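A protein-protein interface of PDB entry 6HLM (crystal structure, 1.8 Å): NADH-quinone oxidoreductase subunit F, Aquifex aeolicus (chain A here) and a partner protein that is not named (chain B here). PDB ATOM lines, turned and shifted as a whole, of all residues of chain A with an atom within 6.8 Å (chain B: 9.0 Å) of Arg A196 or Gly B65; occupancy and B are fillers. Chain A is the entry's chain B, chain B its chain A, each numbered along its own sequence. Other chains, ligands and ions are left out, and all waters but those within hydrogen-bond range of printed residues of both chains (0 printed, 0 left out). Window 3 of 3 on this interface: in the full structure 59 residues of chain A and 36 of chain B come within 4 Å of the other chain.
NE2 of His B62 sits at hydrogen-bond distance from O of Gly A194, at 2.8 Å. The side-chain hydroxyl of Ser A191 sits at hydrogen-bond distance from the side-chain hydroxyl of Tyr B70, at 2.9 Å. The backbone carbonyl oxygen of Lys A195 lies within hydrogen-bond range of the side-chain hydroxyl of Tyr B70, at 2.9 Å. The side-chain hydroxyl (OH) of Tyr B70 sits at hydrogen-bond distance from the backbone NH (N) of Gly A197, at 3.2 Å.
The side-chain carboxylate (OE2) of Glu A190 lies within salt-bridge range of the side-chain amino group (NZ) of Lys A195, 2.8 Å away.
Among the printed residues, pairs that only touch across the chains: Gly A197 with Phe B69 (3.3 Å), Gly A194 with Arg B27 (3.4 Å), Ser A191 with Leu B31 (3.4 Å), His A198 with Phe B69 (3.5 Å), Gly A194 with Ile B30 (3.6 Å), Arg A196 with Gly B65 (3.6 Å), Arg A196 with Phe B69 (3.7 Å), Arg A196 with Tyr B70 (3.7 Å), Cys A182 with Tyr B70 (3.7 Å), Lys A195 with His B62 (3.8 Å) and Gly A194 with Val B66 (3.96 Å).
Of the printed residues of chain B, Cys A182 touches Tyr B70. Glu A190 touches none of the printed residues of chain B. Arg A196 touches just these residues of chain B: Gly B65 (3.6 Å), Phe B69 (3.7 Å) and Tyr B70 (3.7 Å). Gly A197 touches just these residues of chain B: Phe B69 (3.3 Å) and Tyr B70 (3.2 Å). Printed residues of chain B within 4 Å of His A198: Phe B69 (3.5 Å). Pro B59 touches none of the printed residues of chain A. Of the printed residues of chain A, His B62 touches Gly A194 and Lys A195. Of the printed residues of chain A, Phe B69 touches Arg A196 (3.7 Å), Gly A197 (3.3 Å) and His A198 (3.5 Å). The nearest printed residue of chain A that does not touch Gly B65 is Lys A195 (7.2 Å).
Of the 20 printed residues of chain B, 8 touch a printed residue of chain A. Printed residues of chain A that touch a printed residue of chain B: Cys A182, Ser A191, Gly A194, Lys A195, Arg A196, Gly A197 and His A198. Among the printed residues, no Asp or Glu carboxylate lies within 4 Å of a Lys or Arg side-chain nitrogen of the other chain.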
ATOM      1  N   CYS A 182      27.621 -19.995  13.000  1.00  0.00           N
ATOM      2  CA  CYS A 182      26.236 -20.406  13.262  1.00  0.00           C
ATOM      3  C   CYS A 182      25.988 -20.845  14.719  1.00  0.00           C
ATOM      4  O   CYS A 182      24.871 -21.187  15.062  1.00  0.00           O
ATOM      5  CB  CYS A 182      25.766 -21.454  12.260  1.00  0.00           C
ATOM      6  SG  CYS A 182      25.492 -20.777  10.614  1.00  0.00           S
ATOM      7  N   THR A 186      22.241 -15.317  17.000  1.00  0.00           N
ATOM      8  CA  THR A 186      21.461 -14.650  15.950  1.00  0.00           C
ATOM      9  C   THR A 186      21.772 -15.219  14.551  1.00  0.00           C
ATOM     10  O   THR A 186      20.859 -15.310  13.748  1.00  0.00           O
ATOM     11  CB  THR A 186      21.563 -13.119  16.041  1.00  0.00           C
ATOM     12  OG1 THR A 186      22.894 -12.695  15.754  1.00  0.00           O
ATOM     13  CG2 THR A 186      21.142 -12.601  17.425  1.00  0.00           C
ATOM     14  N   ALA A 187      23.019 -15.620  14.274  1.00  0.00           N
ATOM     15  CA  ALA A 187      23.381 -16.274  13.005  1.00  0.00           C
ATOM     16  C   ALA A 187      22.725 -17.685  12.970  1.00  0.00           C
ATOM     17  O   ALA A 187      22.283 -18.148  11.916  1.00  0.00           O
ATOM     18  CB  ALA A 187      24.897 -16.419  12.896  1.00  0.00           C
ATOM     19  N   ILE A 189      19.833 -18.442  14.383  1.00  0.00           N
ATOM     20  CA  ILE A 189      18.452 -18.107  14.024  1.00  0.00           C
ATOM     21  C   ILE A 189      18.335 -17.830  12.498  1.00  0.00           C
ATOM     22  O   ILE A 189      17.433 -18.371  11.849  1.00  0.00           O
ATOM     23  CB  ILE A 189      17.909 -16.942  14.888  1.00  0.00           C
ATOM     24  CG1 ILE A 189      17.657 -17.453  16.345  1.00  0.00           C
ATOM     25  CG2 ILE A 189      16.591 -16.372  14.282  1.00  0.00           C
ATOM     26  CD1 ILE A 189      17.618 -16.358  17.436  1.00  0.00           C
ATOM     27  N   GLU A 190      19.250 -17.027  11.933  1.00  0.00           N
ATOM     28  CA  GLU A 190      19.240 -16.758  10.469  1.00  0.00           C
ATOM     29  C   GLU A 190      19.314 -18.094   9.677  1.00  0.00           C
ATOM     30  O   GLU A 190      18.579 -18.282   8.704  1.00  0.00           O
ATOM     31  CB  GLU A 190      20.406 -15.835  10.078  1.00  0.00           C
ATOM     32  CG  GLU A 190      20.193 -14.373  10.493  1.00  0.00           C
ATOM     33  CD  GLU A 190      19.093 -13.637   9.737  1.00  0.00           C
ATOM     34  OE1 GLU A 190      18.235 -13.001  10.387  1.00  0.00           O
ATOM     35  OE2 GLU A 190      19.086 -13.701   8.493  1.00  0.00           O
ATOM     36  N   SER A 191      20.164 -19.035  10.138  1.00  0.00           N
ATOM     37  CA  SER A 191      20.304 -20.349   9.510  1.00  0.00           C
ATOM     38  C   SER A 191      19.011 -21.179   9.646  1.00  0.00           C
ATOM     39  O   SER A 191      18.600 -21.845   8.690  1.00  0.00           O
ATOM     40  CB  SER A 191      21.508 -21.088  10.070  1.00  0.00           C
ATOM     41  OG  SER A 191      21.798 -22.218   9.258  1.00  0.00           O
ATOM     42  N   GLY A 194      16.525 -20.456   7.081  1.00  0.00           N
ATOM     43  CA  GLY A 194      16.912 -20.898   5.748  1.00  0.00           C
ATOM     44  C   GLY A 194      17.832 -19.951   4.995  1.00  0.00           C
ATOM     45  O   GLY A 194      17.900 -19.993   3.764  1.00  0.00           O
ATOM     46  N   LYS A 195      18.562 -19.114   5.731  1.00  0.00           N
ATOM     47  CA  LYS A 195      19.457 -18.123   5.153  1.00  0.00           C
ATOM     48  C   LYS A 195      20.901 -18.387   5.497  1.00  0.00           C
ATOM     49  O   LYS A 195      21.210 -19.340   6.238  1.00  0.00           O
ATOM     50  CB  LYS A 195      19.047 -16.707   5.613  1.00  0.00           C
ATOM     51  CG  LYS A 195      17.689 -16.249   5.043  1.00  0.00           C
ATOM     52  CD  LYS A 195      17.221 -14.931   5.662  1.00  0.00           C
ATOM     53  CE  LYS A 195      16.608 -15.137   7.027  1.00  0.00           C
ATOM     54  NZ  LYS A 195      16.345 -13.849   7.739  1.00  0.00           N
ATOM     55  N   ARG A 196      21.807 -17.522   4.991  1.00  0.00           N
ATOM     56  CA  ARG A 196      23.230 -17.588   5.360  1.00  0.00           C
ATOM     57  C   ARG A 196      23.317 -17.179   6.855  1.00  0.00           C
ATOM     58  O   ARG A 196      22.478 -16.409   7.343  1.00  0.00           O
ATOM     59  CB  ARG A 196      24.059 -16.636   4.491  1.00  0.00           C
ATOM     60  CG  ARG A 196      24.101 -17.018   2.997  1.00  0.00           C
ATOM     61  CD  ARG A 196      24.747 -15.912   2.159  1.00  0.00           C
ATOM     62  NE  ARG A 196      23.905 -14.719   2.124  1.00  0.00           N
ATOM     63  CZ  ARG A 196      24.305 -13.517   1.710  1.00  0.00           C
ATOM     64  NH1 ARG A 196      25.553 -13.329   1.296  1.00  0.00           N
ATOM     65  NH2 ARG A 196      23.465 -12.496   1.716  1.00  0.00           N
ATOM     66  N   GLY A 197      24.283 -17.740   7.564  1.00  0.00           N
ATOM     67  CA  GLY A 197      24.469 -17.499   8.995  1.00  0.00           C
ATOM     68  C   GLY A 197      25.182 -16.197   9.266  1.00  0.00           C
ATOM     69  O   GLY A 197      26.358 -16.192   9.619  1.00  0.00           O
ATOM     70  N   HIS A 198      24.464 -15.087   9.094  1.00  0.00           N
ATOM     71  CA  HIS A 198      24.993 -13.759   9.346  1.00  0.00           C
ATOM     72  C   HIS A 198      24.431 -13.218  10.661  1.00  0.00           C
ATOM     73  O   HIS A 198      23.224 -13.040  10.778  1.00  0.00           O
ATOM     74  CB  HIS A 198      24.671 -12.801   8.173  1.00  0.00           C
ATOM     75  CG  HIS A 198      25.408 -13.094   6.893  1.00  0.00           C
ATOM     76  ND1 HIS A 198      24.956 -12.610   5.682  1.00  0.00           N
ATOM     77  CD2 HIS A 198      26.560 -13.770   6.684  1.00  0.00           C
ATOM     78  CE1 HIS A 198      25.842 -13.000   4.780  1.00  0.00           C
ATOM     79  NE2 HIS A 198      26.822 -13.705   5.334  1.00  0.00           N
ATOM     80  N   PRO A 199      25.290 -12.913  11.652  1.00  0.00           N
ATOM     81  CA  PRO A 199      24.793 -12.354  12.916  1.00  0.00           C
ATOM     82  C   PRO A 199      24.017 -11.061  12.732  1.00  0.00           C
ATOM     83  O   PRO A 199      24.274 -10.306  11.785  1.00  0.00           O
ATOM     84  CB  PRO A 199      26.072 -12.101  13.713  1.00  0.00           C
ATOM     85  CG  PRO A 199      26.998 -13.136  13.232  1.00  0.00           C
ATOM     86  CD  PRO A 199      26.743 -13.169  11.730  1.00  0.00           C
ATOM     87  N   ARG B  27      11.355 -23.330   3.397  1.00  0.00           N
ATOM     88  CA  ARG B  27      12.705 -22.758   3.273  1.00  0.00           C
ATOM     89  C   ARG B  27      13.668 -23.182   4.392  1.00  0.00           C
ATOM     90  O   ARG B  27      14.888 -23.136   4.198  1.00  0.00           O
ATOM     91  CB  ARG B  27      12.661 -21.229   3.115  1.00  0.00           C
ATOM     92  CG  ARG B  27      12.071 -20.440   4.288  1.00  0.00           C
ATOM     93  CD  ARG B  27      11.865 -19.016   3.790  1.00  0.00           C
ATOM     94  NE  ARG B  27      11.216 -18.099   4.730  1.00  0.00           N
ATOM     95  CZ  ARG B  27       9.900 -17.982   4.902  1.00  0.00           C
ATOM     96  NH1 ARG B  27       9.065 -18.792   4.267  1.00  0.00           N
ATOM     97  NH2 ARG B  27       9.411 -17.075   5.740  1.00  0.00           N
ATOM     98  N   ILE B  30      16.477 -26.025   3.606  1.00  0.00           N
ATOM     99  CA  ILE B  30      17.555 -25.794   2.625  1.00  0.00           C
ATOM    100  C   ILE B  30      18.844 -26.596   2.922  1.00  0.00           C
ATOM    101  O   ILE B  30      19.377 -27.227   2.008  1.00  0.00           O
ATOM    102  CB  ILE B  30      17.855 -24.283   2.386  1.00  0.00           C
ATOM    103  CG1 ILE B  30      18.819 -24.094   1.168  1.00  0.00           C
ATOM    104  CG2 ILE B  30      18.371 -23.555   3.660  1.00  0.00           C
ATOM    105  CD1 ILE B  30      18.737 -22.736   0.449  1.00  0.00           C
ATOM    106  N   LEU B  31      19.339 -26.576   4.167  1.00  0.00           N
ATOM    107  CA  LEU B  31      20.591 -27.273   4.485  1.00  0.00           C
ATOM    108  C   LEU B  31      20.439 -28.782   4.473  1.00  0.00           C
ATOM    109  O   LEU B  31      21.324 -29.467   3.977  1.00  0.00           O
ATOM    110  CB  LEU B  31      21.207 -26.793   5.800  1.00  0.00           C
ATOM    111  CG  LEU B  31      21.473 -25.257   5.863  1.00  0.00           C
ATOM    112  CD1 LEU B  31      22.181 -24.897   7.169  1.00  0.00           C
ATOM    113  CD2 LEU B  31      22.264 -24.771   4.664  1.00  0.00           C
ATOM    114  N   LEU B  34      20.433 -29.823   0.815  1.00  0.00           N
ATOM    115  CA  LEU B  34      21.777 -29.759   0.231  1.00  0.00           C
ATOM    116  C   LEU B  34      22.653 -30.905   0.744  1.00  0.00           C
ATOM    117  O   LEU B  34      23.379 -31.497  -0.054  1.00  0.00           O
ATOM    118  CB  LEU B  34      22.430 -28.380   0.446  1.00  0.00           C
ATOM    119  CG  LEU B  34      21.843 -27.252  -0.398  1.00  0.00           C
ATOM    120  CD1 LEU B  34      22.233 -25.908   0.163  1.00  0.00           C
ATOM    121  CD2 LEU B  34      22.266 -27.376  -1.867  1.00  0.00           C
ATOM    122  N   LEU B  49      20.631 -26.859  -8.425  1.00  0.00           N
ATOM    123  CA  LEU B  49      20.266 -25.662  -7.667  1.00  0.00           C
ATOM    124  C   LEU B  49      18.919 -25.051  -8.067  1.00  0.00           C
ATOM    125  O   LEU B  49      18.145 -24.682  -7.175  1.00  0.00           O
ATOM    126  CB  LEU B  49      21.396 -24.629  -7.708  1.00  0.00           C
ATOM    127  CG  LEU B  49      22.694 -25.061  -6.978  1.00  0.00           C
ATOM    128  CD1 LEU B  49      23.592 -23.876  -6.726  1.00  0.00           C
ATOM    129  CD2 LEU B  49      22.386 -25.734  -5.639  1.00  0.00           C
ATOM    130  N   PRO B  59      14.195 -17.864  -4.498  1.00  0.00           N
ATOM    131  CA  PRO B  59      14.862 -17.485  -5.750  1.00  0.00           C
ATOM    132  C   PRO B  59      16.158 -18.279  -5.893  1.00  0.00           C
ATOM    133  O   PRO B  59      16.761 -18.641  -4.880  1.00  0.00           O
ATOM    134  CB  PRO B  59      15.150 -15.990  -5.573  1.00  0.00           C
ATOM    135  CG  PRO B  59      14.451 -15.575  -4.313  1.00  0.00           C
ATOM    136  CD  PRO B  59      14.291 -16.789  -3.492  1.00  0.00           C
ATOM    137  N   LEU B  60      16.580 -18.561  -7.142  1.00  0.00           N
ATOM    138  CA  LEU B  60      17.820 -19.292  -7.411  1.00  0.00           C
ATOM    139  C   LEU B  60      19.028 -18.611  -6.761  1.00  0.00           C
ATOM    140  O   LEU B  60      19.889 -19.307  -6.224  1.00  0.00           O
ATOM    141  CB  LEU B  60      18.039 -19.489  -8.929  1.00  0.00           C
ATOM    142  CG  LEU B  60      19.365 -20.141  -9.382  1.00  0.00           C
ATOM    143  CD1 LEU B  60      19.538 -21.554  -8.804  1.00  0.00           C
ATOM    144  CD2 LEU B  60      19.461 -20.169 -10.900  1.00  0.00           C
ATOM    145  N   ASN B  61      19.072 -17.257  -6.786  1.00  0.00           N
ATOM    146  CA  ASN B  61      20.168 -16.492  -6.179  1.00  0.00           C
ATOM    147  C   ASN B  61      20.305 -16.769  -4.673  1.00  0.00           C
ATOM    148  O   ASN B  61      21.430 -16.807  -4.170  1.00  0.00           O
ATOM    149  CB  ASN B  61      20.073 -14.989  -6.486  1.00  0.00           C
ATOM    150  CG  ASN B  61      19.301 -14.166  -5.481  1.00  0.00           C
ATOM    151  OD1 ASN B  61      19.859 -13.673  -4.493  1.00  0.00           O
ATOM    152  ND2 ASN B  61      18.004 -14.012  -5.694  1.00  0.00           N
ATOM    153  N   HIS B  62      19.166 -16.960  -3.961  1.00  0.00           N
ATOM    154  CA  HIS B  62      19.174 -17.266  -2.513  1.00  0.00           C
ATOM    155  C   HIS B  62      19.879 -18.620  -2.284  1.00  0.00           C
ATOM    156  O   HIS B  62      20.765 -18.719  -1.426  1.00  0.00           O
ATOM    157  CB  HIS B  62      17.724 -17.279  -1.977  1.00  0.00           C
ATOM    158  CG  HIS B  62      17.561 -17.552  -0.510  1.00  0.00           C
ATOM    159  ND1 HIS B  62      16.671 -16.825   0.256  1.00  0.00           N
ATOM    160  CD2 HIS B  62      18.140 -18.496   0.275  1.00  0.00           C
ATOM    161  CE1 HIS B  62      16.751 -17.336   1.472  1.00  0.00           C
ATOM    162  NE2 HIS B  62      17.634 -18.332   1.531  1.00  0.00           N
ATOM    163  N   VAL B  63      19.497 -19.652  -3.062  1.00  0.00           N
ATOM    164  CA  VAL B  63      20.068 -21.006  -2.958  1.00  0.00           C
ATOM    165  C   VAL B  63      21.584 -20.999  -3.270  1.00  0.00           C
ATOM    166  O   VAL B  63      22.354 -21.559  -2.494  1.00  0.00           O
ATOM    167  CB  VAL B  63      19.261 -22.041  -3.797  1.00  0.00           C
ATOM    168  CG1 VAL B  63      19.909 -23.427  -3.774  1.00  0.00           C
ATOM    169  CG2 VAL B  63      17.810 -22.116  -3.321  1.00  0.00           C
ATOM    170  N   GLU B  64      22.002 -20.327  -4.358  1.00  0.00           N
ATOM    171  CA  GLU B  64      23.418 -20.195  -4.746  1.00  0.00           C
ATOM    172  C   GLU B  64      24.260 -19.542  -3.626  1.00  0.00           C
ATOM    173  O   GLU B  64      25.354 -20.022  -3.329  1.00  0.00           O
ATOM    174  CB  GLU B  64      23.562 -19.389  -6.063  1.00  0.00           C
ATOM    175  CG  GLU B  64      23.011 -20.115  -7.284  1.00  0.00           C
ATOM    176  CD  GLU B  64      23.067 -19.350  -8.594  1.00  0.00           C
ATOM    177  OE1 GLU B  64      22.970 -18.101  -8.570  1.00  0.00           O
ATOM    178  OE2 GLU B  64      23.167 -20.010  -9.654  1.00  0.00           O
ATOM    179  N   GLY B  65      23.732 -18.478  -3.012  1.00  0.00           N
ATOM    180  CA  GLY B  65      24.384 -17.792  -1.897  1.00  0.00           C
ATOM    181  C   GLY B  65      24.551 -18.691  -0.681  1.00  0.00           C
ATOM    182  O   GLY B  65      25.602 -18.692  -0.028  1.00  0.00           O
ATOM    183  N   VAL B  66      23.524 -19.519  -0.399  1.00  0.00           N
ATOM    184  CA  VAL B  66      23.556 -20.476   0.708  1.00  0.00           C
ATOM    185  C   VAL B  66      24.621 -21.559   0.461  1.00  0.00           C
ATOM    186  O   VAL B  66      25.418 -21.817   1.355  1.00  0.00           O
ATOM    187  CB  VAL B  66      22.147 -21.043   1.038  1.00  0.00           C
ATOM    188  CG1 VAL B  66      22.230 -22.302   1.919  1.00  0.00           C
ATOM    189  CG2 VAL B  66      21.291 -19.975   1.720  1.00  0.00           C
ATOM    190  N   VAL B  67      24.669 -22.149  -0.758  1.00  0.00           N
ATOM    191  CA  VAL B  67      25.672 -23.176  -1.108  1.00  0.00           C
ATOM    192  C   VAL B  67      27.103 -22.631  -0.937  1.00  0.00           C
ATOM    193  O   VAL B  67      27.956 -23.338  -0.411  1.00  0.00           O
ATOM    194  CB  VAL B  67      25.465 -23.778  -2.528  1.00  0.00           C
ATOM    195  CG1 VAL B  67      26.542 -24.809  -2.849  1.00  0.00           C
ATOM    196  CG2 VAL B  67      24.091 -24.406  -2.661  1.00  0.00           C
ATOM    197  N   ALA B  68      27.345 -21.387  -1.383  1.00  0.00           N
ATOM    198  CA  ALA B  68      28.640 -20.694  -1.309  1.00  0.00           C
ATOM    199  C   ALA B  68      29.078 -20.428   0.141  1.00  0.00           C
ATOM    200  O   ALA B  68      30.264 -20.541   0.456  1.00  0.00           O
ATOM    201  CB  ALA B  68      28.571 -19.381  -2.080  1.00  0.00           C
ATOM    202  N   PHE B  69      28.121 -20.062   1.014  1.00  0.00           N
ATOM    203  CA  PHE B  69      28.392 -19.736   2.415  1.00  0.00           C
ATOM    204  C   PHE B  69      28.862 -20.924   3.270  1.00  0.00           C
ATOM    205  O   PHE B  69      29.799 -20.782   4.054  1.00  0.00           O
ATOM    206  CB  PHE B  69      27.164 -19.050   3.066  1.00  0.00           C
ATOM    207  CG  PHE B  69      27.400 -18.589   4.495  1.00  0.00           C
ATOM    208  CD1 PHE B  69      27.100 -19.419   5.573  1.00  0.00           C
ATOM    209  CD2 PHE B  69      27.903 -17.314   4.760  1.00  0.00           C
ATOM    210  CE1 PHE B  69      27.348 -19.006   6.890  1.00  0.00           C
ATOM    211  CE2 PHE B  69      28.143 -16.901   6.080  1.00  0.00           C
ATOM    212  CZ  PHE B  69      27.886 -17.763   7.128  1.00  0.00           C
ATOM    213  N   TYR B  70      28.161 -22.061   3.169  1.00  0.00           N
ATOM    214  CA  TYR B  70      28.382 -23.228   4.014  1.00  0.00           C
ATOM    215  C   TYR B  70      29.486 -24.144   3.483  1.00  0.00           C
ATOM    216  O   TYR B  70      29.356 -24.726   2.400  1.00  0.00           O
ATOM    217  CB  TYR B  70      27.043 -23.938   4.235  1.00  0.00           C
ATOM    218  CG  TYR B  70      26.077 -23.098   5.049  1.00  0.00           C
ATOM    219  CD1 TYR B  70      25.075 -22.352   4.430  1.00  0.00           C
ATOM    220  CD2 TYR B  70      26.171 -23.037   6.437  1.00  0.00           C
ATOM    221  CE1 TYR B  70      24.178 -21.588   5.177  1.00  0.00           C
ATOM    222  CE2 TYR B  70      25.271 -22.291   7.194  1.00  0.00           C
ATOM    223  CZ  TYR B  70      24.273 -21.570   6.560  1.00  0.00           C
ATOM    224  OH  TYR B  70      23.386 -20.839   7.318  1.00  0.00           O
ATOM    225  N   ASP B  71      30.584 -24.249   4.267  1.00  0.00           N
ATOM    226  CA  ASP B  71      31.839 -24.950   3.952  1.00  0.00           C
ATOM    227  C   ASP B  71      31.714 -26.430   3.584  1.00  0.00           C
ATOM    228  O   ASP B  71      32.498 -26.906   2.762  1.00  0.00           O
ATOM    229  CB  ASP B  71      32.854 -24.800   5.095  1.00  0.00           C
ATOM    230  CG  ASP B  71      34.298 -25.097   4.694  1.00  0.00           C
ATOM    231  OD1 ASP B  71      34.887 -26.075   5.244  1.00  0.00           O
ATOM    232  OD2 ASP B  71      34.849 -24.346   3.853  1.00  0.00           O
ATOM    233  N   PHE B  73      29.562 -27.913   1.699  1.00  0.00           N
ATOM    234  CA  PHE B  73      29.105 -28.130   0.320  1.00  0.00           C
ATOM    235  C   PHE B  73      30.191 -27.909  -0.724  1.00  0.00           C
ATOM    236  O   PHE B  73      30.908 -26.913  -0.686  1.00  0.00           O
ATOM    237  CB  PHE B  73      27.842 -27.314   0.011  1.00  0.00           C
ATOM    238  CG  PHE B  73      26.760 -27.539   1.041  1.00  0.00           C
ATOM    239  CD1 PHE B  73      26.411 -28.827   1.439  1.00  0.00           C
ATOM    240  CD2 PHE B  73      26.054 -26.470   1.574  1.00  0.00           C
ATOM    241  CE1 PHE B  73      25.432 -29.036   2.421  1.00  0.00           C
ATOM    242  CE2 PHE B  73      25.052 -26.680   2.526  1.00  0.00           C
ATOM    243  CZ  PHE B  73      24.754 -27.962   2.949  1.00  0.00           C
ATOM    244  N   ARG B  75      30.777 -27.802  -4.844  1.00  0.00           N
ATOM    245  CA  ARG B  75      30.177 -27.644  -6.175  1.00  0.00           C
ATOM    246  C   ARG B  75      31.122 -28.073  -7.302  1.00  0.00           C
ATOM    247  O   ARG B  75      30.702 -28.079  -8.460  1.00  0.00           O
ATOM    248  CB  ARG B  75      29.793 -26.170  -6.399  1.00  0.00           C
ATOM    249  CG  ARG B  75      28.412 -25.785  -5.889  1.00  0.00           C
ATOM    250  CD  ARG B  75      28.095 -24.325  -6.185  1.00  0.00           C
ATOM    251  NE  ARG B  75      29.021 -23.428  -5.495  1.00  0.00           N
ATOM    252  CZ  ARG B  75      28.783 -22.147  -5.221  1.00  0.00           C
ATOM    253  NH1 ARG B  75      29.697 -21.416  -4.596  1.00  0.00           N
ATOM    254  NH2 ARG B  75      27.621 -21.590  -5.558  1.00  0.00           N
